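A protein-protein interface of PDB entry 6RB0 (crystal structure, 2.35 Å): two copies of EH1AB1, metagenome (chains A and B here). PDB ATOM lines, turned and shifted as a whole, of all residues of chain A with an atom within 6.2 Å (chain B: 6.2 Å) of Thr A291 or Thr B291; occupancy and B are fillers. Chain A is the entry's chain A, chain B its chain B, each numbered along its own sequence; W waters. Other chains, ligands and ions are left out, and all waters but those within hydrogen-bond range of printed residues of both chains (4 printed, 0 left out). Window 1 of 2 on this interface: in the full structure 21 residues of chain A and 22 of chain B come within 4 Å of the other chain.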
ATOM      1  N   ALA A 262     -11.403   2.263 -10.600  1.00  0.00           N
ATOM      2  CA  ALA A 262     -11.843   3.556 -10.053  1.00  0.00           C
ATOM      3  C   ALA A 262     -13.283   3.477  -9.565  1.00  0.00           C
ATOM      4  O   ALA A 262     -14.083   2.723 -10.125  1.00  0.00           O
ATOM      5  CB  ALA A 262     -11.687   4.628 -11.101  1.00  0.00           C
ATOM      6  N   PHE A 263     -13.563   4.300  -8.566  1.00  0.00           N
ATOM      7  CA  PHE A 263     -14.911   4.740  -8.158  1.00  0.00           C
ATOM      8  C   PHE A 263     -14.953   6.253  -8.344  1.00  0.00           C
ATOM      9  O   PHE A 263     -14.054   6.936  -7.850  1.00  0.00           O
ATOM     10  CB  PHE A 263     -15.160   4.291  -6.723  1.00  0.00           C
ATOM     11  CG  PHE A 263     -16.410   4.847  -6.104  1.00  0.00           C
ATOM     12  CD1 PHE A 263     -17.616   4.186  -6.240  1.00  0.00           C
ATOM     13  CD2 PHE A 263     -16.363   6.011  -5.351  1.00  0.00           C
ATOM     14  CE1 PHE A 263     -18.759   4.695  -5.649  1.00  0.00           C
ATOM     15  CE2 PHE A 263     -17.506   6.507  -4.752  1.00  0.00           C
ATOM     16  CZ  PHE A 263     -18.701   5.853  -4.905  1.00  0.00           C
ATOM     17  N   VAL A 264     -15.935   6.760  -9.083  1.00  0.00           N
ATOM     18  CA  VAL A 264     -16.065   8.216  -9.361  1.00  0.00           C
ATOM     19  C   VAL A 264     -17.473   8.646  -8.967  1.00  0.00           C
ATOM     20  O   VAL A 264     -18.436   8.082  -9.499  1.00  0.00           O
ATOM     21  CB  VAL A 264     -15.762   8.543 -10.831  1.00  0.00           C
ATOM     22  CG1 VAL A 264     -15.793  10.043 -11.074  1.00  0.00           C
ATOM     23  CG2 VAL A 264     -14.439   7.945 -11.271  1.00  0.00           C
ATOM     24  N   LEU A 265     -17.568   9.594  -8.043  1.00  0.00           N
ATOM     25  CA  LEU A 265     -18.852  10.088  -7.498  1.00  0.00           C
ATOM     26  C   LEU A 265     -18.995  11.562  -7.869  1.00  0.00           C
ATOM     27  O   LEU A 265     -18.033  12.323  -7.657  1.00  0.00           O
ATOM     28  CB  LEU A 265     -18.856   9.899  -5.982  1.00  0.00           C
ATOM     29  CG  LEU A 265     -20.157  10.312  -5.299  1.00  0.00           C
ATOM     30  CD1 LEU A 265     -20.417   9.485  -4.052  1.00  0.00           C
ATOM     31  CD2 LEU A 265     -20.153  11.794  -4.984  1.00  0.00           C
ATOM     32  N   ALA A 280     -14.667   9.652 -15.531  1.00  0.00           N
ATOM     33  CA  ALA A 280     -15.212   8.276 -15.481  1.00  0.00           C
ATOM     34  C   ALA A 280     -15.365   7.731 -16.910  1.00  0.00           C
ATOM     35  O   ALA A 280     -14.987   6.565 -17.150  1.00  0.00           O
ATOM     36  CB  ALA A 280     -16.519   8.264 -14.726  1.00  0.00           C
ATOM     37  N   ILE A 284     -13.709   4.382 -18.533  1.00  0.00           N
ATOM     38  CA  ILE A 284     -14.558   3.296 -19.095  1.00  0.00           C
ATOM     39  C   ILE A 284     -14.098   2.997 -20.524  1.00  0.00           C
ATOM     40  O   ILE A 284     -13.883   1.811 -20.815  1.00  0.00           O
ATOM     41  CB  ILE A 284     -16.054   3.657 -19.022  1.00  0.00           C
ATOM     42  CG1 ILE A 284     -16.551   3.674 -17.574  1.00  0.00           C
ATOM     43  CG2 ILE A 284     -16.874   2.705 -19.881  1.00  0.00           C
ATOM     44  CD1 ILE A 284     -17.802   4.483 -17.357  1.00  0.00           C
ATOM     45  N   LYS A 289     -11.765  -0.889 -15.126  1.00  0.00           N
ATOM     46  CA  LYS A 289     -12.929  -1.212 -14.266  1.00  0.00           C
ATOM     47  C   LYS A 289     -13.300   0.074 -13.531  1.00  0.00           C
ATOM     48  O   LYS A 289     -12.443   0.619 -12.815  1.00  0.00           O
ATOM     49  CB  LYS A 289     -12.654  -2.344 -13.273  1.00  0.00           C
ATOM     50  CG  LYS A 289     -13.807  -2.579 -12.301  1.00  0.00           C
ATOM     51  CD  LYS A 289     -13.474  -3.539 -11.215  1.00  0.00           C
ATOM     52  CE  LYS A 289     -13.385  -4.957 -11.740  1.00  0.00           C
ATOM     53  NZ  LYS A 289     -12.767  -5.901 -10.778  1.00  0.00           N
ATOM     54  N   THR A 290     -14.506   0.575 -13.763  1.00  0.00           N
ATOM     55  CA  THR A 290     -14.928   1.922 -13.312  1.00  0.00           C
ATOM     56  C   THR A 290     -16.349   1.827 -12.774  1.00  0.00           C
ATOM     57  O   THR A 290     -17.214   1.292 -13.484  1.00  0.00           O
ATOM     58  CB  THR A 290     -14.840   2.969 -14.433  1.00  0.00           C
ATOM     59  OG1 THR A 290     -13.530   2.895 -15.000  1.00  0.00           O
ATOM     60  CG2 THR A 290     -15.139   4.374 -13.945  1.00  0.00           C
ATOM     61  N   THR A 291     -16.540   2.321 -11.555  1.00  0.00           N
ATOM     62  CA  THR A 291     -17.865   2.565 -10.948  1.00  0.00           C
ATOM     63  C   THR A 291     -18.082   4.076 -10.957  1.00  0.00           C
ATOM     64  O   THR A 291     -17.199   4.804 -10.457  1.00  0.00           O
ATOM     65  CB  THR A 291     -17.948   1.944  -9.553  1.00  0.00           C
ATOM     66  OG1 THR A 291     -17.603   0.564  -9.702  1.00  0.00           O
ATOM     67  CG2 THR A 291     -19.314   2.100  -8.930  1.00  0.00           C
ATOM     68  N   TYR A 292     -19.166   4.521 -11.581  1.00  0.00           N
ATOM     69  CA  TYR A 292     -19.584   5.940 -11.611  1.00  0.00           C
ATOM     70  C   TYR A 292     -20.910   6.045 -10.869  1.00  0.00           C
ATOM     71  O   TYR A 292     -21.796   5.226 -11.148  1.00  0.00           O
ATOM     72  CB  TYR A 292     -19.748   6.468 -13.038  1.00  0.00           C
ATOM     73  CG  TYR A 292     -20.345   7.850 -13.036  1.00  0.00           C
ATOM     74  CD1 TYR A 292     -19.597   8.945 -12.632  1.00  0.00           C
ATOM     75  CD2 TYR A 292     -21.679   8.056 -13.333  1.00  0.00           C
ATOM     76  CE1 TYR A 292     -20.145  10.216 -12.586  1.00  0.00           C
ATOM     77  CE2 TYR A 292     -22.244   9.319 -13.287  1.00  0.00           C
ATOM     78  CZ  TYR A 292     -21.476  10.401 -12.908  1.00  0.00           C
ATOM     79  OH  TYR A 292     -22.030  11.643 -12.862  1.00  0.00           O
ATOM     80  N   VAL A 293     -21.055   6.998  -9.956  1.00  0.00           N
ATOM     81  CA  VAL A 293     -22.370   7.226  -9.293  1.00  0.00           C
ATOM     82  C   VAL A 293     -22.648   8.722  -9.307  1.00  0.00           C
ATOM     83  O   VAL A 293     -21.719   9.494  -9.039  1.00  0.00           O
ATOM     84  CB  VAL A 293     -22.430   6.639  -7.870  1.00  0.00           C
ATOM     85  CG1 VAL A 293     -21.310   7.151  -6.992  1.00  0.00           C
ATOM     86  CG2 VAL A 293     -23.774   6.896  -7.211  1.00  0.00           C
ATOM     87  N   ASN A 294     -23.878   9.104  -9.632  1.00  0.00           N
ATOM     88  CA  ASN A 294     -24.325  10.505  -9.472  1.00  0.00           C
ATOM     89  C   ASN A 294     -25.389  10.551  -8.377  1.00  0.00           C
ATOM     90  O   ASN A 294     -26.361   9.770  -8.451  1.00  0.00           O
ATOM     91  CB  ASN A 294     -24.808  11.130 -10.776  1.00  0.00           C
ATOM     92  CG  ASN A 294     -25.157  12.588 -10.589  1.00  0.00           C
ATOM     93  OD1 ASN A 294     -26.318  12.977 -10.689  1.00  0.00           O
ATOM     94  ND2 ASN A 294     -24.167  13.391 -10.252  1.00  0.00           N
ATOM     95  N   TYR A 295     -25.173  11.425  -7.398  1.00  0.00           N
ATOM     96  CA  TYR A 295     -26.116  11.741  -6.300  1.00  0.00           C
ATOM     97  C   TYR A 295     -26.859  13.015  -6.680  1.00  0.00           C
ATOM     98  O   TYR A 295     -26.390  14.122  -6.427  1.00  0.00           O
ATOM     99  CB  TYR A 295     -25.362  11.869  -4.976  1.00  0.00           C
ATOM    100  CG  TYR A 295     -25.080  10.552  -4.301  1.00  0.00           C
ATOM    101  CD1 TYR A 295     -24.100   9.698  -4.774  1.00  0.00           C
ATOM    102  CD2 TYR A 295     -25.803  10.156  -3.186  1.00  0.00           C
ATOM    103  CE1 TYR A 295     -23.850   8.477  -4.163  1.00  0.00           C
ATOM    104  CE2 TYR A 295     -25.564   8.938  -2.565  1.00  0.00           C
ATOM    105  CZ  TYR A 295     -24.589   8.096  -3.059  1.00  0.00           C
ATOM    106  OH  TYR A 295     -24.355   6.897  -2.454  1.00  0.00           O
ATOM    107  N   GLU A 318     -21.383   3.943   0.273  1.00  0.00           N
ATOM    108  CA  GLU A 318     -21.246   3.428  -1.110  1.00  0.00           C
ATOM    109  C   GLU A 318     -19.764   3.418  -1.503  1.00  0.00           C
ATOM    110  O   GLU A 318     -19.288   2.381  -1.936  1.00  0.00           O
ATOM    111  CB  GLU A 318     -22.086   4.235  -2.088  1.00  0.00           C
ATOM    112  CG  GLU A 318     -21.979   3.676  -3.492  1.00  0.00           C
ATOM    113  CD  GLU A 318     -22.985   4.179  -4.508  1.00  0.00           C
ATOM    114  OE1 GLU A 318     -23.773   5.104  -4.175  1.00  0.00           O
ATOM    115  OE2 GLU A 318     -22.960   3.647  -5.642  1.00  0.00           O
ATOM    116  N   VAL A 322     -17.867  -0.232  -2.149  1.00  0.00           N
ATOM    117  CA  VAL A 322     -17.271  -0.530  -3.484  1.00  0.00           C
ATOM    118  C   VAL A 322     -15.774  -0.819  -3.330  1.00  0.00           C
ATOM    119  O   VAL A 322     -15.289  -1.772  -3.970  1.00  0.00           O
ATOM    120  CB  VAL A 322     -17.520   0.597  -4.496  1.00  0.00           C
ATOM    121  CG1 VAL A 322     -16.722   0.379  -5.770  1.00  0.00           C
ATOM    122  CG2 VAL A 322     -18.995   0.717  -4.820  1.00  0.00           C
ATOM    123  N   ALA B 262     -30.775   3.145  -8.850  1.00  0.00           N
ATOM    124  CA  ALA B 262     -30.364   1.979  -9.658  1.00  0.00           C
ATOM    125  C   ALA B 262     -28.879   1.696  -9.490  1.00  0.00           C
ATOM    126  O   ALA B 262     -28.094   2.626  -9.308  1.00  0.00           O
ATOM    127  CB  ALA B 262     -30.696   2.200 -11.112  1.00  0.00           C
ATOM    128  N   PHE B 263     -28.545   0.425  -9.626  1.00  0.00           N
ATOM    129  CA  PHE B 263     -27.185  -0.102  -9.863  1.00  0.00           C
ATOM    130  C   PHE B 263     -27.231  -0.816 -11.211  1.00  0.00           C
ATOM    131  O   PHE B 263     -28.099  -1.659 -11.409  1.00  0.00           O
ATOM    132  CB  PHE B 263     -26.795  -1.013  -8.699  1.00  0.00           C
ATOM    133  CG  PHE B 263     -25.512  -1.769  -8.895  1.00  0.00           C
ATOM    134  CD1 PHE B 263     -24.295  -1.193  -8.562  1.00  0.00           C
ATOM    135  CD2 PHE B 263     -25.524  -3.044  -9.430  1.00  0.00           C
ATOM    136  CE1 PHE B 263     -23.114  -1.892  -8.749  1.00  0.00           C
ATOM    137  CE2 PHE B 263     -24.343  -3.744  -9.603  1.00  0.00           C
ATOM    138  CZ  PHE B 263     -23.140  -3.167  -9.267  1.00  0.00           C
ATOM    139  N   VAL B 264     -26.355  -0.447 -12.136  1.00  0.00           N
ATOM    140  CA  VAL B 264     -26.320  -1.054 -13.495  1.00  0.00           C
ATOM    141  C   VAL B 264     -24.901  -1.541 -13.750  1.00  0.00           C
ATOM    142  O   VAL B 264     -23.976  -0.726 -13.700  1.00  0.00           O
ATOM    143  CB  VAL B 264     -26.790  -0.073 -14.582  1.00  0.00           C
ATOM    144  CG1 VAL B 264     -26.858  -0.758 -15.940  1.00  0.00           C
ATOM    145  CG2 VAL B 264     -28.130   0.544 -14.225  1.00  0.00           C
ATOM    146  N   LEU B 265     -24.765  -2.838 -13.997  1.00  0.00           N
ATOM    147  CA  LEU B 265     -23.465  -3.503 -14.217  1.00  0.00           C
ATOM    148  C   LEU B 265     -23.441  -4.045 -15.640  1.00  0.00           C
ATOM    149  O   LEU B 265     -24.421  -4.700 -16.045  1.00  0.00           O
ATOM    150  CB  LEU B 265     -23.304  -4.621 -13.187  1.00  0.00           C
ATOM    151  CG  LEU B 265     -21.974  -5.361 -13.260  1.00  0.00           C
ATOM    152  CD1 LEU B 265     -21.567  -5.878 -11.895  1.00  0.00           C
ATOM    153  CD2 LEU B 265     -22.023  -6.486 -14.292  1.00  0.00           C
ATOM    154  N   ALA B 280     -28.334   3.076 -18.052  1.00  0.00           N
ATOM    155  CA  ALA B 280     -27.735   3.856 -16.946  1.00  0.00           C
ATOM    156  C   ALA B 280     -27.686   5.338 -17.338  1.00  0.00           C
ATOM    157  O   ALA B 280     -28.038   6.189 -16.489  1.00  0.00           O
ATOM    158  CB  ALA B 280     -26.369   3.314 -16.627  1.00  0.00           C
ATOM    159  N   ILE B 284     -29.355   8.489 -15.359  1.00  0.00           N
ATOM    160  CA  ILE B 284     -28.515   9.623 -14.875  1.00  0.00           C
ATOM    161  C   ILE B 284     -29.100  10.934 -15.410  1.00  0.00           C
ATOM    162  O   ILE B 284     -29.297  11.850 -14.587  1.00  0.00           O
ATOM    163  CB  ILE B 284     -27.040   9.432 -15.266  1.00  0.00           C
ATOM    164  CG1 ILE B 284     -26.419   8.265 -14.488  1.00  0.00           C
ATOM    165  CG2 ILE B 284     -26.262  10.731 -15.073  1.00  0.00           C
ATOM    166  CD1 ILE B 284     -25.167   7.686 -15.128  1.00  0.00           C
ATOM    167  N   LYS B 289     -30.755   8.688  -8.957  1.00  0.00           N
ATOM    168  CA  LYS B 289     -29.502   8.257  -8.293  1.00  0.00           C
ATOM    169  C   LYS B 289     -29.106   6.925  -8.929  1.00  0.00           C
ATOM    170  O   LYS B 289     -29.907   5.977  -8.863  1.00  0.00           O
ATOM    171  CB  LYS B 289     -29.690   8.163  -6.777  1.00  0.00           C
ATOM    172  CG  LYS B 289     -28.409   7.968  -5.982  1.00  0.00           C
ATOM    173  CD  LYS B 289     -28.269   6.604  -5.348  1.00  0.00           C
ATOM    174  CE  LYS B 289     -26.819   6.169  -5.266  1.00  0.00           C
ATOM    175  NZ  LYS B 289     -26.645   4.950  -4.438  1.00  0.00           N
ATOM    176  N   THR B 290     -27.953   6.879  -9.587  1.00  0.00           N
ATOM    177  CA  THR B 290     -27.552   5.747 -10.458  1.00  0.00           C
ATOM    178  C   THR B 290     -26.077   5.431 -10.226  1.00  0.00           C
ATOM    179  O   THR B 290     -25.260   6.364 -10.273  1.00  0.00           O
ATOM    180  CB  THR B 290     -27.811   6.037 -11.944  1.00  0.00           C
ATOM    181  OG1 THR B 290     -29.173   6.439 -12.094  1.00  0.00           O
ATOM    182  CG2 THR B 290     -27.530   4.845 -12.841  1.00  0.00           C
ATOM    183  N   THR B 291     -25.783   4.159  -9.980  1.00  0.00           N
ATOM    184  CA  THR B 291     -24.413   3.602  -9.987  1.00  0.00           C
ATOM    185  C   THR B 291     -24.279   2.753 -11.248  1.00  0.00           C
ATOM    186  O   THR B 291     -25.126   1.856 -11.450  1.00  0.00           O
ATOM    187  CB  THR B 291     -24.131   2.811  -8.707  1.00  0.00           C
ATOM    188  OG1 THR B 291     -24.438   3.673  -7.613  1.00  0.00           O
ATOM    189  CG2 THR B 291     -22.698   2.338  -8.628  1.00  0.00           C
ATOM    190  N   TYR B 292     -23.300   3.076 -12.088  1.00  0.00           N
ATOM    191  CA  TYR B 292     -22.946   2.290 -13.294  1.00  0.00           C
ATOM    192  C   TYR B 292     -21.558   1.701 -13.078  1.00  0.00           C
ATOM    193  O   TYR B 292     -20.679   2.446 -12.649  1.00  0.00           O
ATOM    194  CB  TYR B 292     -22.934   3.141 -14.562  1.00  0.00           C
ATOM    195  CG  TYR B 292     -22.396   2.370 -15.739  1.00  0.00           C
ATOM    196  CD1 TYR B 292     -23.158   1.380 -16.335  1.00  0.00           C
ATOM    197  CD2 TYR B 292     -21.108   2.560 -16.204  1.00  0.00           C
ATOM    198  CE1 TYR B 292     -22.679   0.632 -17.394  1.00  0.00           C
ATOM    199  CE2 TYR B 292     -20.610   1.823 -17.269  1.00  0.00           C
ATOM    200  CZ  TYR B 292     -21.394   0.848 -17.860  1.00  0.00           C
ATOM    201  OH  TYR B 292     -20.921   0.094 -18.900  1.00  0.00           O
ATOM    202  N   VAL B 293     -21.360   0.414 -13.344  1.00  0.00           N
ATOM    203  CA  VAL B 293     -19.999  -0.183 -13.286  1.00  0.00           C
ATOM    204  C   VAL B 293     -19.814  -1.032 -14.539  1.00  0.00           C
ATOM    205  O   VAL B 293     -20.747  -1.750 -14.913  1.00  0.00           O
ATOM    206  CB  VAL B 293     -19.772  -0.994 -11.997  1.00  0.00           C
ATOM    207  CG1 VAL B 293     -20.832  -2.069 -11.793  1.00  0.00           C
ATOM    208  CG2 VAL B 293     -18.388  -1.618 -11.967  1.00  0.00           C
ATOM    209  N   ASN B 294     -18.648  -0.940 -15.164  1.00  0.00           N
ATOM    210  CA  ASN B 294     -18.260  -1.867 -16.251  1.00  0.00           C
ATOM    211  C   ASN B 294     -17.106  -2.743 -15.760  1.00  0.00           C
ATOM    212  O   ASN B 294     -16.114  -2.204 -15.246  1.00  0.00           O
ATOM    213  CB  ASN B 294     -17.918  -1.144 -17.547  1.00  0.00           C
ATOM    214  CG  ASN B 294     -17.645  -2.127 -18.663  1.00  0.00           C
ATOM    215  OD1 ASN B 294     -16.526  -2.195 -19.162  1.00  0.00           O
ATOM    216  ND2 ASN B 294     -18.637  -2.930 -19.016  1.00  0.00           N
ATOM    217  N   TYR B 295     -17.279  -4.053 -15.897  1.00  0.00           N
ATOM    218  CA  TYR B 295     -16.260  -5.091 -15.619  1.00  0.00           C
ATOM    219  C   TYR B 295     -15.620  -5.474 -16.947  1.00  0.00           C
ATOM    220  O   TYR B 295     -16.110  -6.355 -17.651  1.00  0.00           O
ATOM    221  CB  TYR B 295     -16.891  -6.278 -14.889  1.00  0.00           C
ATOM    222  CG  TYR B 295     -17.036  -6.068 -13.405  1.00  0.00           C
ATOM    223  CD1 TYR B 295     -18.000  -5.225 -12.883  1.00  0.00           C
ATOM    224  CD2 TYR B 295     -16.191  -6.709 -12.520  1.00  0.00           C
ATOM    225  CE1 TYR B 295     -18.115  -5.021 -11.519  1.00  0.00           C
ATOM    226  CE2 TYR B 295     -16.291  -6.516 -11.154  1.00  0.00           C
ATOM    227  CZ  TYR B 295     -17.252  -5.661 -10.650  1.00  0.00           C
ATOM    228  OH  TYR B 295     -17.349  -5.478  -9.304  1.00  0.00           O
ATOM    229  N   GLU B 318     -19.857  -6.186  -5.020  1.00  0.00           N
ATOM    230  CA  GLU B 318     -20.091  -4.768  -5.375  1.00  0.00           C
ATOM    231  C   GLU B 318     -21.602  -4.518  -5.434  1.00  0.00           C
ATOM    232  O   GLU B 318     -22.057  -3.596  -4.762  1.00  0.00           O
ATOM    233  CB  GLU B 318     -19.400  -4.378  -6.670  1.00  0.00           C
ATOM    234  CG  GLU B 318     -19.607  -2.907  -6.974  1.00  0.00           C
ATOM    235  CD  GLU B 318     -18.823  -2.334  -8.138  1.00  0.00           C
ATOM    236  OE1 GLU B 318     -18.073  -3.099  -8.797  1.00  0.00           O
ATOM    237  OE2 GLU B 318     -18.950  -1.107  -8.361  1.00  0.00           O
ATOM    238  N   VAL B 322     -23.375  -1.980  -2.652  1.00  0.00           N
ATOM    239  CA  VAL B 322     -24.072  -0.746  -3.126  1.00  0.00           C
ATOM    240  C   VAL B 322     -25.534  -0.774  -2.673  1.00  0.00           C
ATOM    241  O   VAL B 322     -26.042   0.281  -2.232  1.00  0.00           O
ATOM    242  CB  VAL B 322     -23.976  -0.573  -4.649  1.00  0.00           C
ATOM    243  CG1 VAL B 322     -24.918   0.513  -5.157  1.00  0.00           C
ATOM    244  CG2 VAL B 322     -22.545  -0.292  -5.061  1.00  0.00           C
HETATM  245  O   HOH W   1     -16.002  -3.133  -6.310  1.00  0.00           O
HETATM  246  O   HOH W   2     -25.774   2.782  -2.862  1.00  0.00           O
HETATM  247  O   HOH W   3     -28.656  11.435 -11.780  1.00  0.00           O
HETATM  248  O   HOH W   4     -14.334  -0.151 -18.729  1.00  0.00           O
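Ala A262 touches none of the printed residues of chain B.
Thr A291 touches just these residues of chain B: Thr B291, Tyr B292, Val B293 and Glu B318.
Of the printed residues of chain B, Val A293 touches Lys B289, Thr B290 and Thr B291.
Printed residues of chain B within 4 Å of Glu A318: Lys B289, Thr B291 and Val B322.
Of the printed residues of chain B, Val A322 touches Glu B318 (3.7 Å) and Val B322 (3.7 Å).
Printed residues of chain A within 4 Å of Ile B284: Tyr A292.
Of chain A, only Thr A291, Tyr A292, Val A293 and Glu A318 come within 4 Å of Thr B291.
Of the printed residues of chain A, Tyr B292 touches Ile A284, Thr A290, Thr A291 and Tyr A292.
The nearest residue of chain B that does not touch Thr A291 is Asn B294 (5.3 Å).
The nearest residue of chain A that does not touch Thr B291 is Asn A294 (5.3 Å).
The nearest printed residue of chain A that does not touch Tyr B295 is Thr A290 (5.8 Å).
The backbone NH (N) of Asn B294 is in hydrogen-bond range of the backbone carbonyl oxygen (O) of Thr A290 (3.1 Å).
The side-chain hydroxyl (OG1) of Thr A291 is in hydrogen-bond range of the side-chain carboxylate (OE2) of Glu B318, 2.5 Å away.
N of Tyr A292 is in hydrogen-bond range of O of Tyr B292.
N of Asn A294 sits at hydrogen-bond distance from O of Thr B290, at 3.1 Å.
The side-chain amino group (NZ) of Lys B289 is in salt-bridge range of the side-chain carboxylate (OE1) of Glu A318 (2.9 Å).
The side-chain carboxylate (OE2) of Glu A318 sits at hydrogen-bond distance from the side-chain hydroxyl (OG1) of Thr B291, at 2.5 Å.
O of Ala A262 is in hydrogen-bond range of N of Thr A291 (2.9 Å).
The backbone NH of Val A264 is in hydrogen-bond range of the backbone carbonyl oxygen of Thr A291, at 2.7 Å.
The backbone carbonyl oxygen (O) of Val A264 is in hydrogen-bond range of the backbone NH (N) of Val A293, at 2.9 Å.
The backbone NH (N) of Thr B291 is in hydrogen-bond range of the backbone carbonyl oxygen (O) of Ala B262 (2.9 Å).
N of Val B264 is in hydrogen-bond range of O of Thr B291 (2.7 Å).
N of Val B293 is in hydrogen-bond range of O of Val B264, at 2.9 Å.
Water W2 lies within hydrogen-bond range of O of Val B322 (2.6 Å), NZ of Lys B289 (2.8 Å) and OE1 of Glu A318 (3.3 Å).
Water W1 bridges O of Val A322 (2.8 Å) and OE1 of Glu B318 (3.2 Å).
Water W4 lies within hydrogen-bond range of the backbone carbonyl oxygen (O) of Ile A284 (2.9 Å) and the side-chain amide oxygen (OD1) of Asn B294 (3.0 Å).
Water W3 bridges the backbone carbonyl oxygen (O) of Ile B284 and the side-chain amide oxygen (OD1) of Asn A294.
Lys A289 touches Tyr B295, and with the chains exchanged Tyr A295 touches Lys B289.
Thr A291 touches its own counterpart, Thr B291.
Thr A291 touches Tyr B292, and with the chains exchanged Tyr A292 touches Thr B291.
Val B322 touches its own counterpart, Val A322.
15 positions are printed for both chains.
Of the 25 pairs that touch across the chains among the printed residues, 23 have their exchanged pair printed and touching as well.
Tyr B292 touches Ile A284.
Lys A289 touches Asn B294 (CA to O, 3.5 Å).
Lys A289 touches Tyr B295.
O of Tyr B292 touches CA of Thr A291 (3.3 Å).
Thr A291 touches Val B293.
Tyr A292 touches Thr B290 (O to O, 3.7 Å).
Tyr A292 touches Thr B291.
CE of Lys B289 touches CG2 of Val A293 (3.7 Å).
Thr B291 touches Val A293.
Tyr A295 touches Lys B289.
Of the 15 printed residues of chain A, 10 touch a printed residue of chain B.
Hydrophobic or aromatic side chains of chain A within 4 Å of the printed part of chain B: Ile A284, Tyr A292, Val A293, Tyr A295 and Val A322.
Of the 15 printed residues of chain B, 10 touch a printed residue of chain A.
Along chain B the printed residues that touch a printed residue of chain A span positions 284 to 322.
Among the printed residues, Asp or Glu carboxylates within 4 Å of a Lys or Arg side-chain nitrogen of the other chain: Glu A318 with Lys B289.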
